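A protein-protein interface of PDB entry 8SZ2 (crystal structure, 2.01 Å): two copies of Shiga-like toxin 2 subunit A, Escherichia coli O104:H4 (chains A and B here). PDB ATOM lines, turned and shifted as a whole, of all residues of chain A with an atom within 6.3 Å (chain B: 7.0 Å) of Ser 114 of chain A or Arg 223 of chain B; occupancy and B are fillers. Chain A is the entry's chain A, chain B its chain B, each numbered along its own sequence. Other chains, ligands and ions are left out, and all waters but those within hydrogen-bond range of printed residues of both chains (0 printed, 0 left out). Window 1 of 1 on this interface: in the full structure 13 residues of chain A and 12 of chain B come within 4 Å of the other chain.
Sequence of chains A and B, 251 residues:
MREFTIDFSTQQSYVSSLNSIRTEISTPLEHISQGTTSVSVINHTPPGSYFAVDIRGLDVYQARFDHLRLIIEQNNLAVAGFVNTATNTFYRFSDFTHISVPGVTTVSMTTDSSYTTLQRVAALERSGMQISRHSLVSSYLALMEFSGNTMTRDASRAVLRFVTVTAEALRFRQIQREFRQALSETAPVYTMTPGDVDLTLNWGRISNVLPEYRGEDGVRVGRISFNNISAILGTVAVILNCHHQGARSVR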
ATOM      1  N   ASP A  95     -17.945   2.588   2.187  1.00  0.00           N
ATOM      2  CA  ASP A  95     -16.547   2.991   2.164  1.00  0.00           C
ATOM      3  C   ASP A  95     -16.195   3.767   0.896  1.00  0.00           C
ATOM      4  O   ASP A  95     -15.012   3.974   0.608  1.00  0.00           O
ATOM      5  CB  ASP A  95     -15.618   1.778   2.353  1.00  0.00           C
ATOM      6  CG  ASP A  95     -15.996   0.588   1.485  1.00  0.00           C
ATOM      7  OD1 ASP A  95     -17.167   0.492   1.062  1.00  0.00           O
ATOM      8  OD2 ASP A  95     -15.121  -0.268   1.239  1.00  0.00           O
ATOM      9  N   ASP A 112     -20.425  -2.023   3.645  1.00  0.00           N
ATOM     10  CA  ASP A 112     -19.159  -1.754   2.976  1.00  0.00           C
ATOM     11  C   ASP A 112     -18.858  -2.828   1.927  1.00  0.00           C
ATOM     12  O   ASP A 112     -19.515  -3.870   1.849  1.00  0.00           O
ATOM     13  CB  ASP A 112     -18.019  -1.683   3.990  1.00  0.00           C
ATOM     14  CG  ASP A 112     -17.718  -3.025   4.607  1.00  0.00           C
ATOM     15  OD1 ASP A 112     -18.338  -3.358   5.638  1.00  0.00           O
ATOM     16  OD2 ASP A 112     -16.882  -3.764   4.046  1.00  0.00           O
ATOM     17  N   SER A 113     -17.826  -2.570   1.124  1.00  0.00           N
ATOM     18  CA  SER A 113     -17.489  -3.406  -0.026  1.00  0.00           C
ATOM     19  C   SER A 113     -16.551  -4.558   0.287  1.00  0.00           C
ATOM     20  O   SER A 113     -16.210  -5.303  -0.638  1.00  0.00           O
ATOM     21  CB  SER A 113     -16.823  -2.564  -1.116  1.00  0.00           C
ATOM     22  OG  SER A 113     -15.549  -2.132  -0.648  1.00  0.00           O
ATOM     23  N   SER A 114     -16.071  -4.702   1.525  1.00  0.00           N
ATOM     24  CA  SER A 114     -15.057  -5.722   1.774  1.00  0.00           C
ATOM     25  C   SER A 114     -15.609  -7.119   1.500  1.00  0.00           C
ATOM     26  O   SER A 114     -16.816  -7.378   1.602  1.00  0.00           O
ATOM     27  CB  SER A 114     -14.518  -5.640   3.205  1.00  0.00           C
ATOM     28  OG  SER A 114     -15.453  -6.118   4.139  1.00  0.00           O
ATOM     29  N   TYR A 115     -14.698  -8.026   1.144  1.00  0.00           N
ATOM     30  CA  TYR A 115     -15.072  -9.420   0.951  1.00  0.00           C
ATOM     31  C   TYR A 115     -15.597 -10.042   2.239  1.00  0.00           C
ATOM     32  O   TYR A 115     -16.529 -10.853   2.193  1.00  0.00           O
ATOM     33  CB  TYR A 115     -13.875 -10.207   0.406  1.00  0.00           C
ATOM     34  CG  TYR A 115     -13.616  -9.963  -1.084  1.00  0.00           C
ATOM     35  CD1 TYR A 115     -14.651 -10.014  -1.998  1.00  0.00           C
ATOM     36  CD2 TYR A 115     -12.334  -9.691  -1.561  1.00  0.00           C
ATOM     37  CE1 TYR A 115     -14.437  -9.806  -3.352  1.00  0.00           C
ATOM     38  CE2 TYR A 115     -12.105  -9.480  -2.923  1.00  0.00           C
ATOM     39  CZ  TYR A 115     -13.162  -9.538  -3.810  1.00  0.00           C
ATOM     40  OH  TYR A 115     -12.961  -9.342  -5.161  1.00  0.00           O
ATOM     41  N   THR A 116     -15.030  -9.677   3.393  1.00  0.00           N
ATOM     42  CA  THR A 116     -15.528 -10.229   4.648  1.00  0.00           C
ATOM     43  C   THR A 116     -17.005  -9.898   4.834  1.00  0.00           C
ATOM     44  O   THR A 116     -17.818 -10.782   5.124  1.00  0.00           O
ATOM     45  CB  THR A 116     -14.693  -9.725   5.828  1.00  0.00           C
ATOM     46  OG1 THR A 116     -13.341 -10.171   5.675  1.00  0.00           O
ATOM     47  CG2 THR A 116     -15.229 -10.301   7.137  1.00  0.00           C
ATOM     48  N   THR A 117     -17.378  -8.635   4.628  1.00  0.00           N
ATOM     49  CA  THR A 117     -18.781  -8.242   4.752  1.00  0.00           C
ATOM     50  C   THR A 117     -19.645  -8.929   3.697  1.00  0.00           C
ATOM     51  O   THR A 117     -20.673  -9.533   4.023  1.00  0.00           O
ATOM     52  CB  THR A 117     -18.894  -6.721   4.647  1.00  0.00           C
ATOM     53  OG1 THR A 117     -18.133  -6.127   5.705  1.00  0.00           O
ATOM     54  CG2 THR A 117     -20.341  -6.254   4.745  1.00  0.00           C
ATOM     55  N   LEU A 118     -19.234  -8.862   2.429  1.00  0.00           N
ATOM     56  CA  LEU A 118     -20.061  -9.406   1.354  1.00  0.00           C
ATOM     57  C   LEU A 118     -20.259 -10.906   1.505  1.00  0.00           C
ATOM     58  O   LEU A 118     -21.362 -11.414   1.282  1.00  0.00           O
ATOM     59  CB  LEU A 118     -19.436  -9.094  -0.004  1.00  0.00           C
ATOM     60  CG  LEU A 118     -19.395  -7.626  -0.420  1.00  0.00           C
ATOM     61  CD1 LEU A 118     -18.700  -7.526  -1.748  1.00  0.00           C
ATOM     62  CD2 LEU A 118     -20.809  -7.044  -0.511  1.00  0.00           C
ATOM     63  N   GLN A 119     -19.206 -11.636   1.890  1.00  0.00           N
ATOM     64  CA  GLN A 119     -19.353 -13.078   2.075  1.00  0.00           C
ATOM     65  C   GLN A 119     -20.241 -13.403   3.276  1.00  0.00           C
ATOM     66  O   GLN A 119     -20.925 -14.436   3.281  1.00  0.00           O
ATOM     67  CB  GLN A 119     -17.979 -13.740   2.227  1.00  0.00           C
ATOM     68  CG  GLN A 119     -17.125 -13.734   0.950  1.00  0.00           C
ATOM     69  CD  GLN A 119     -15.698 -14.221   1.192  1.00  0.00           C
ATOM     70  OE1 GLN A 119     -15.343 -15.336   0.837  1.00  0.00           O
ATOM     71  NE2 GLN A 119     -14.882 -13.382   1.805  1.00  0.00           N
ATOM     72  N   ARG A 120     -20.229 -12.559   4.312  1.00  0.00           N
ATOM     73  CA  ARG A 120     -21.131 -12.782   5.441  1.00  0.00           C
ATOM     74  C   ARG A 120     -22.585 -12.625   5.013  1.00  0.00           C
ATOM     75  O   ARG A 120     -23.410 -13.515   5.247  1.00  0.00           O
ATOM     76  CB  ARG A 120     -20.811 -11.827   6.594  1.00  0.00           C
ATOM     77  CG  ARG A 120     -21.818 -11.917   7.758  1.00  0.00           C
ATOM     78  CD  ARG A 120     -21.547 -10.882   8.862  1.00  0.00           C
ATOM     79  NE  ARG A 120     -21.712  -9.502   8.400  1.00  0.00           N
ATOM     80  CZ  ARG A 120     -22.810  -8.775   8.569  1.00  0.00           C
ATOM     81  NH1 ARG A 120     -23.884  -9.273   9.161  1.00  0.00           N
ATOM     82  NH2 ARG A 120     -22.829  -7.519   8.133  1.00  0.00           N
ATOM     83  N   LEU A 160     -20.496 -10.172  -5.469  1.00  0.00           N
ATOM     84  CA  LEU A 160     -19.310 -11.036  -5.430  1.00  0.00           C
ATOM     85  C   LEU A 160     -18.993 -11.602  -6.813  1.00  0.00           C
ATOM     86  O   LEU A 160     -17.827 -11.623  -7.240  1.00  0.00           O
ATOM     87  CB  LEU A 160     -19.496 -12.176  -4.420  1.00  0.00           C
ATOM     88  CG  LEU A 160     -19.372 -11.796  -2.940  1.00  0.00           C
ATOM     89  CD1 LEU A 160     -19.923 -12.907  -2.037  1.00  0.00           C
ATOM     90  CD2 LEU A 160     -17.921 -11.511  -2.612  1.00  0.00           C
ATOM     91  N   PRO B 194      -9.233 -10.236  17.384  1.00  0.00           N
ATOM     92  CA  PRO B 194      -9.610 -10.191  15.958  1.00  0.00           C
ATOM     93  C   PRO B 194      -9.518  -8.794  15.376  1.00  0.00           C
ATOM     94  O   PRO B 194      -9.036  -8.621  14.248  1.00  0.00           O
ATOM     95  CB  PRO B 194     -11.053 -10.717  15.960  1.00  0.00           C
ATOM     96  CG  PRO B 194     -11.112 -11.608  17.152  1.00  0.00           C
ATOM     97  CD  PRO B 194     -10.229 -10.955  18.196  1.00  0.00           C
ATOM     98  N   GLY B 195      -9.950  -7.788  16.145  1.00  0.00           N
ATOM     99  CA  GLY B 195      -9.767  -6.406  15.732  1.00  0.00           C
ATOM    100  C   GLY B 195      -8.321  -6.055  15.423  1.00  0.00           C
ATOM    101  O   GLY B 195      -8.039  -5.404  14.412  1.00  0.00           O
ATOM    102  N   ASP B 198      -7.396  -7.705  12.176  1.00  0.00           N
ATOM    103  CA  ASP B 198      -8.013  -7.045  11.025  1.00  0.00           C
ATOM    104  C   ASP B 198      -7.285  -5.759  10.640  1.00  0.00           C
ATOM    105  O   ASP B 198      -7.178  -5.443   9.446  1.00  0.00           O
ATOM    106  CB  ASP B 198      -9.487  -6.764  11.308  1.00  0.00           C
ATOM    107  CG  ASP B 198     -10.327  -6.741  10.038  1.00  0.00           C
ATOM    108  OD1 ASP B 198     -10.343  -7.767   9.320  1.00  0.00           O
ATOM    109  OD2 ASP B 198     -10.980  -5.713   9.758  1.00  0.00           O
ATOM    110  N   ASN B 202      -5.267  -4.915   6.841  1.00  0.00           N
ATOM    111  CA  ASN B 202      -5.759  -3.802   6.039  1.00  0.00           C
ATOM    112  C   ASN B 202      -4.818  -2.598   6.051  1.00  0.00           C
ATOM    113  O   ASN B 202      -5.253  -1.473   5.774  1.00  0.00           O
ATOM    114  CB  ASN B 202      -7.148  -3.390   6.529  1.00  0.00           C
ATOM    115  CG  ASN B 202      -8.219  -4.358   6.086  1.00  0.00           C
ATOM    116  OD1 ASN B 202      -8.612  -4.368   4.922  1.00  0.00           O
ATOM    117  ND2 ASN B 202      -8.664  -5.209   6.997  1.00  0.00           N
ATOM    118  N   ARG B 220     -13.908   5.442   6.484  1.00  0.00           N
ATOM    119  CA  ARG B 220     -14.316   4.045   6.413  1.00  0.00           C
ATOM    120  C   ARG B 220     -13.459   3.314   5.386  1.00  0.00           C
ATOM    121  O   ARG B 220     -13.433   3.691   4.209  1.00  0.00           O
ATOM    122  CB  ARG B 220     -15.796   3.936   6.049  1.00  0.00           C
ATOM    123  CG  ARG B 220     -16.302   2.507   5.877  1.00  0.00           C
ATOM    124  CD  ARG B 220     -16.375   1.763   7.198  1.00  0.00           C
ATOM    125  NE  ARG B 220     -17.505   0.842   7.228  1.00  0.00           N
ATOM    126  CZ  ARG B 220     -18.680   1.122   7.771  1.00  0.00           C
ATOM    127  NH1 ARG B 220     -18.909   2.281   8.374  1.00  0.00           N
ATOM    128  NH2 ARG B 220     -19.658   0.223   7.693  1.00  0.00           N
ATOM    129  N   VAL B 221     -12.780   2.259   5.833  1.00  0.00           N
ATOM    130  CA  VAL B 221     -11.986   1.377   4.986  1.00  0.00           C
ATOM    131  C   VAL B 221     -12.512  -0.029   5.247  1.00  0.00           C
ATOM    132  O   VAL B 221     -12.183  -0.636   6.273  1.00  0.00           O
ATOM    133  CB  VAL B 221     -10.486   1.464   5.295  1.00  0.00           C
ATOM    134  CG1 VAL B 221      -9.676   0.848   4.175  1.00  0.00           C
ATOM    135  CG2 VAL B 221     -10.059   2.903   5.545  1.00  0.00           C
ATOM    136  N   GLY B 222     -13.311  -0.556   4.326  1.00  0.00           N
ATOM    137  CA  GLY B 222     -13.913  -1.867   4.527  1.00  0.00           C
ATOM    138  C   GLY B 222     -14.753  -1.911   5.790  1.00  0.00           C
ATOM    139  O   GLY B 222     -15.657  -1.089   5.994  1.00  0.00           O
ATOM    140  N   ARG B 223     -14.449  -2.874   6.663  1.00  0.00           N
ATOM    141  CA  ARG B 223     -15.075  -2.952   7.978  1.00  0.00           C
ATOM    142  C   ARG B 223     -14.431  -2.022   9.005  1.00  0.00           C
ATOM    143  O   ARG B 223     -14.996  -1.850  10.091  1.00  0.00           O
ATOM    144  CB  ARG B 223     -15.035  -4.398   8.493  1.00  0.00           C
ATOM    145  CG  ARG B 223     -15.912  -5.355   7.716  1.00  0.00           C
ATOM    146  CD  ARG B 223     -16.129  -6.682   8.444  1.00  0.00           C
ATOM    147  NE  ARG B 223     -14.887  -7.446   8.503  1.00  0.00           N
ATOM    148  CZ  ARG B 223     -14.145  -7.612   9.592  1.00  0.00           C
ATOM    149  NH1 ARG B 223     -14.505  -7.101  10.757  1.00  0.00           N
ATOM    150  NH2 ARG B 223     -13.012  -8.309   9.511  1.00  0.00           N
ATOM    151  N   ILE B 224     -13.287  -1.416   8.695  1.00  0.00           N
ATOM    152  CA  ILE B 224     -12.610  -0.515   9.625  1.00  0.00           C
ATOM    153  C   ILE B 224     -13.234   0.871   9.525  1.00  0.00           C
ATOM    154  O   ILE B 224     -13.164   1.517   8.474  1.00  0.00           O
ATOM    155  CB  ILE B 224     -11.104  -0.442   9.346  1.00  0.00           C
ATOM    156  CG1 ILE B 224     -10.479  -1.835   9.329  1.00  0.00           C
ATOM    157  CG2 ILE B 224     -10.423   0.406  10.412  1.00  0.00           C
ATOM    158  CD1 ILE B 224     -10.526  -2.514  10.655  1.00  0.00           C
ATOM    159  N   SER B 225     -13.781   1.356  10.635  1.00  0.00           N
ATOM    160  CA  SER B 225     -14.445   2.651  10.690  1.00  0.00           C
ATOM    161  C   SER B 225     -13.764   3.529  11.729  1.00  0.00           C
ATOM    162  O   SER B 225     -13.550   3.099  12.869  1.00  0.00           O
ATOM    163  CB  SER B 225     -15.928   2.475  11.017  1.00  0.00           C
ATOM    164  OG  SER B 225     -16.587   3.721  11.149  1.00  0.00           O
ATOM    165  N   PHE B 226     -13.417   4.746  11.336  1.00  0.00           N
ATOM    166  CA  PHE B 226     -12.867   5.746  12.242  1.00  0.00           C
ATOM    167  C   PHE B 226     -13.863   6.888  12.346  1.00  0.00           C
ATOM    168  O   PHE B 226     -14.137   7.566  11.351  1.00  0.00           O
ATOM    169  CB  PHE B 226     -11.516   6.261  11.752  1.00  0.00           C
ATOM    170  CG  PHE B 226     -10.451   5.207  11.696  1.00  0.00           C
ATOM    171  CD1 PHE B 226      -9.927   4.674  12.863  1.00  0.00           C
ATOM    172  CD2 PHE B 226      -9.981   4.743  10.481  1.00  0.00           C
ATOM    173  CE1 PHE B 226      -8.952   3.701  12.819  1.00  0.00           C
ATOM    174  CE2 PHE B 226      -8.998   3.764  10.433  1.00  0.00           C
ATOM    175  CZ  PHE B 226      -8.482   3.249  11.609  1.00  0.00           C
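No position is printed for both chains. Of the 7 pairs that touch across the chains among the printed residues, none has its exchanged pair printed and touching as well.
Among the printed residues, pairs that only touch across the chains: Thr 117 of chain A with Arg 223 of chain B (3.1 Å), Asp 112 of chain A with Gly 222 of chain B (3.1 Å), Thr 116 of chain A with Arg 223 of chain B (3.2 Å), Asp 95 of chain A with Arg 220 of chain B (3.4 Å), Asp 95 of chain A with Gly 222 of chain B (3.6 Å), Asp 112 of chain A with Arg 223 of chain B (3.7 Å) and Ser 114 of chain A with Arg 223 of chain B (3.7 Å).
Printed residues of chain B that touch a printed residue of chain A: Arg 220, Gly 222 and Arg 223. Printed residues of chain A that touch a printed residue of chain B: Asp 95, Asp 112, Ser 114, Thr 116 and Thr 117. Among the printed residues, no Asp or Glu carboxylate lies within 4 Å of a Lys or Arg side-chain nitrogen of the other chain.
Of the printed residues of chain B, Asp 95 of chain A touches Arg 220 and Gly 222. Ser 114 of chain A touches one residue of chain B. Of the printed residues of chain B, Thr 116 of chain A touches Arg 223. Of the printed residues of chain B, Thr 117 of chain A touches Arg 223 (3.1 Å). Pro 194 of chain B touches none of the printed residues of chain A. Asn 202 of chain B touches none of the printed residues of chain A. Printed residues of chain A within 4 Å of Arg 220 of chain B: Asp 95. Printed residues of chain A within 4 Å of Gly 222 of chain B: Asp 95 and Asp 112. The nearest residue of chain B that does not touch Ser 114 of chain A is Gly 222 of chain B (4.04 Å). The nearest printed residue of chain A that does not touch Arg 223 of chain B is Asp 95 of chain A (6.1 Å).
OD2 of Asp 112 of chain A sits at hydrogen-bond distance from OG of Ser 114 of chain A (2.8 Å). O of Gly 222 of chain B lies within hydrogen-bond range of NE of Arg 220 of chain B. The side-chain carboxylate of Asp 112 of chain A sits at hydrogen-bond distance from the side-chain hydroxyl of Thr 117 of chain A, 2.8 Å away. OG1 of Thr 117 of chain A lies within hydrogen-bond range of OG of Ser 114 of chain A, at 3.1 Å. OG of Ser 113 of chain A is in hydrogen-bond range of OD2 of Asp 95 of chain A, 2.7 Å away. The guanidinium group (NH2) of Arg 223 of chain B is in salt-bridge range of the side-chain carboxylate (OD1) of Asp 198 of chain B (2.7 Å).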
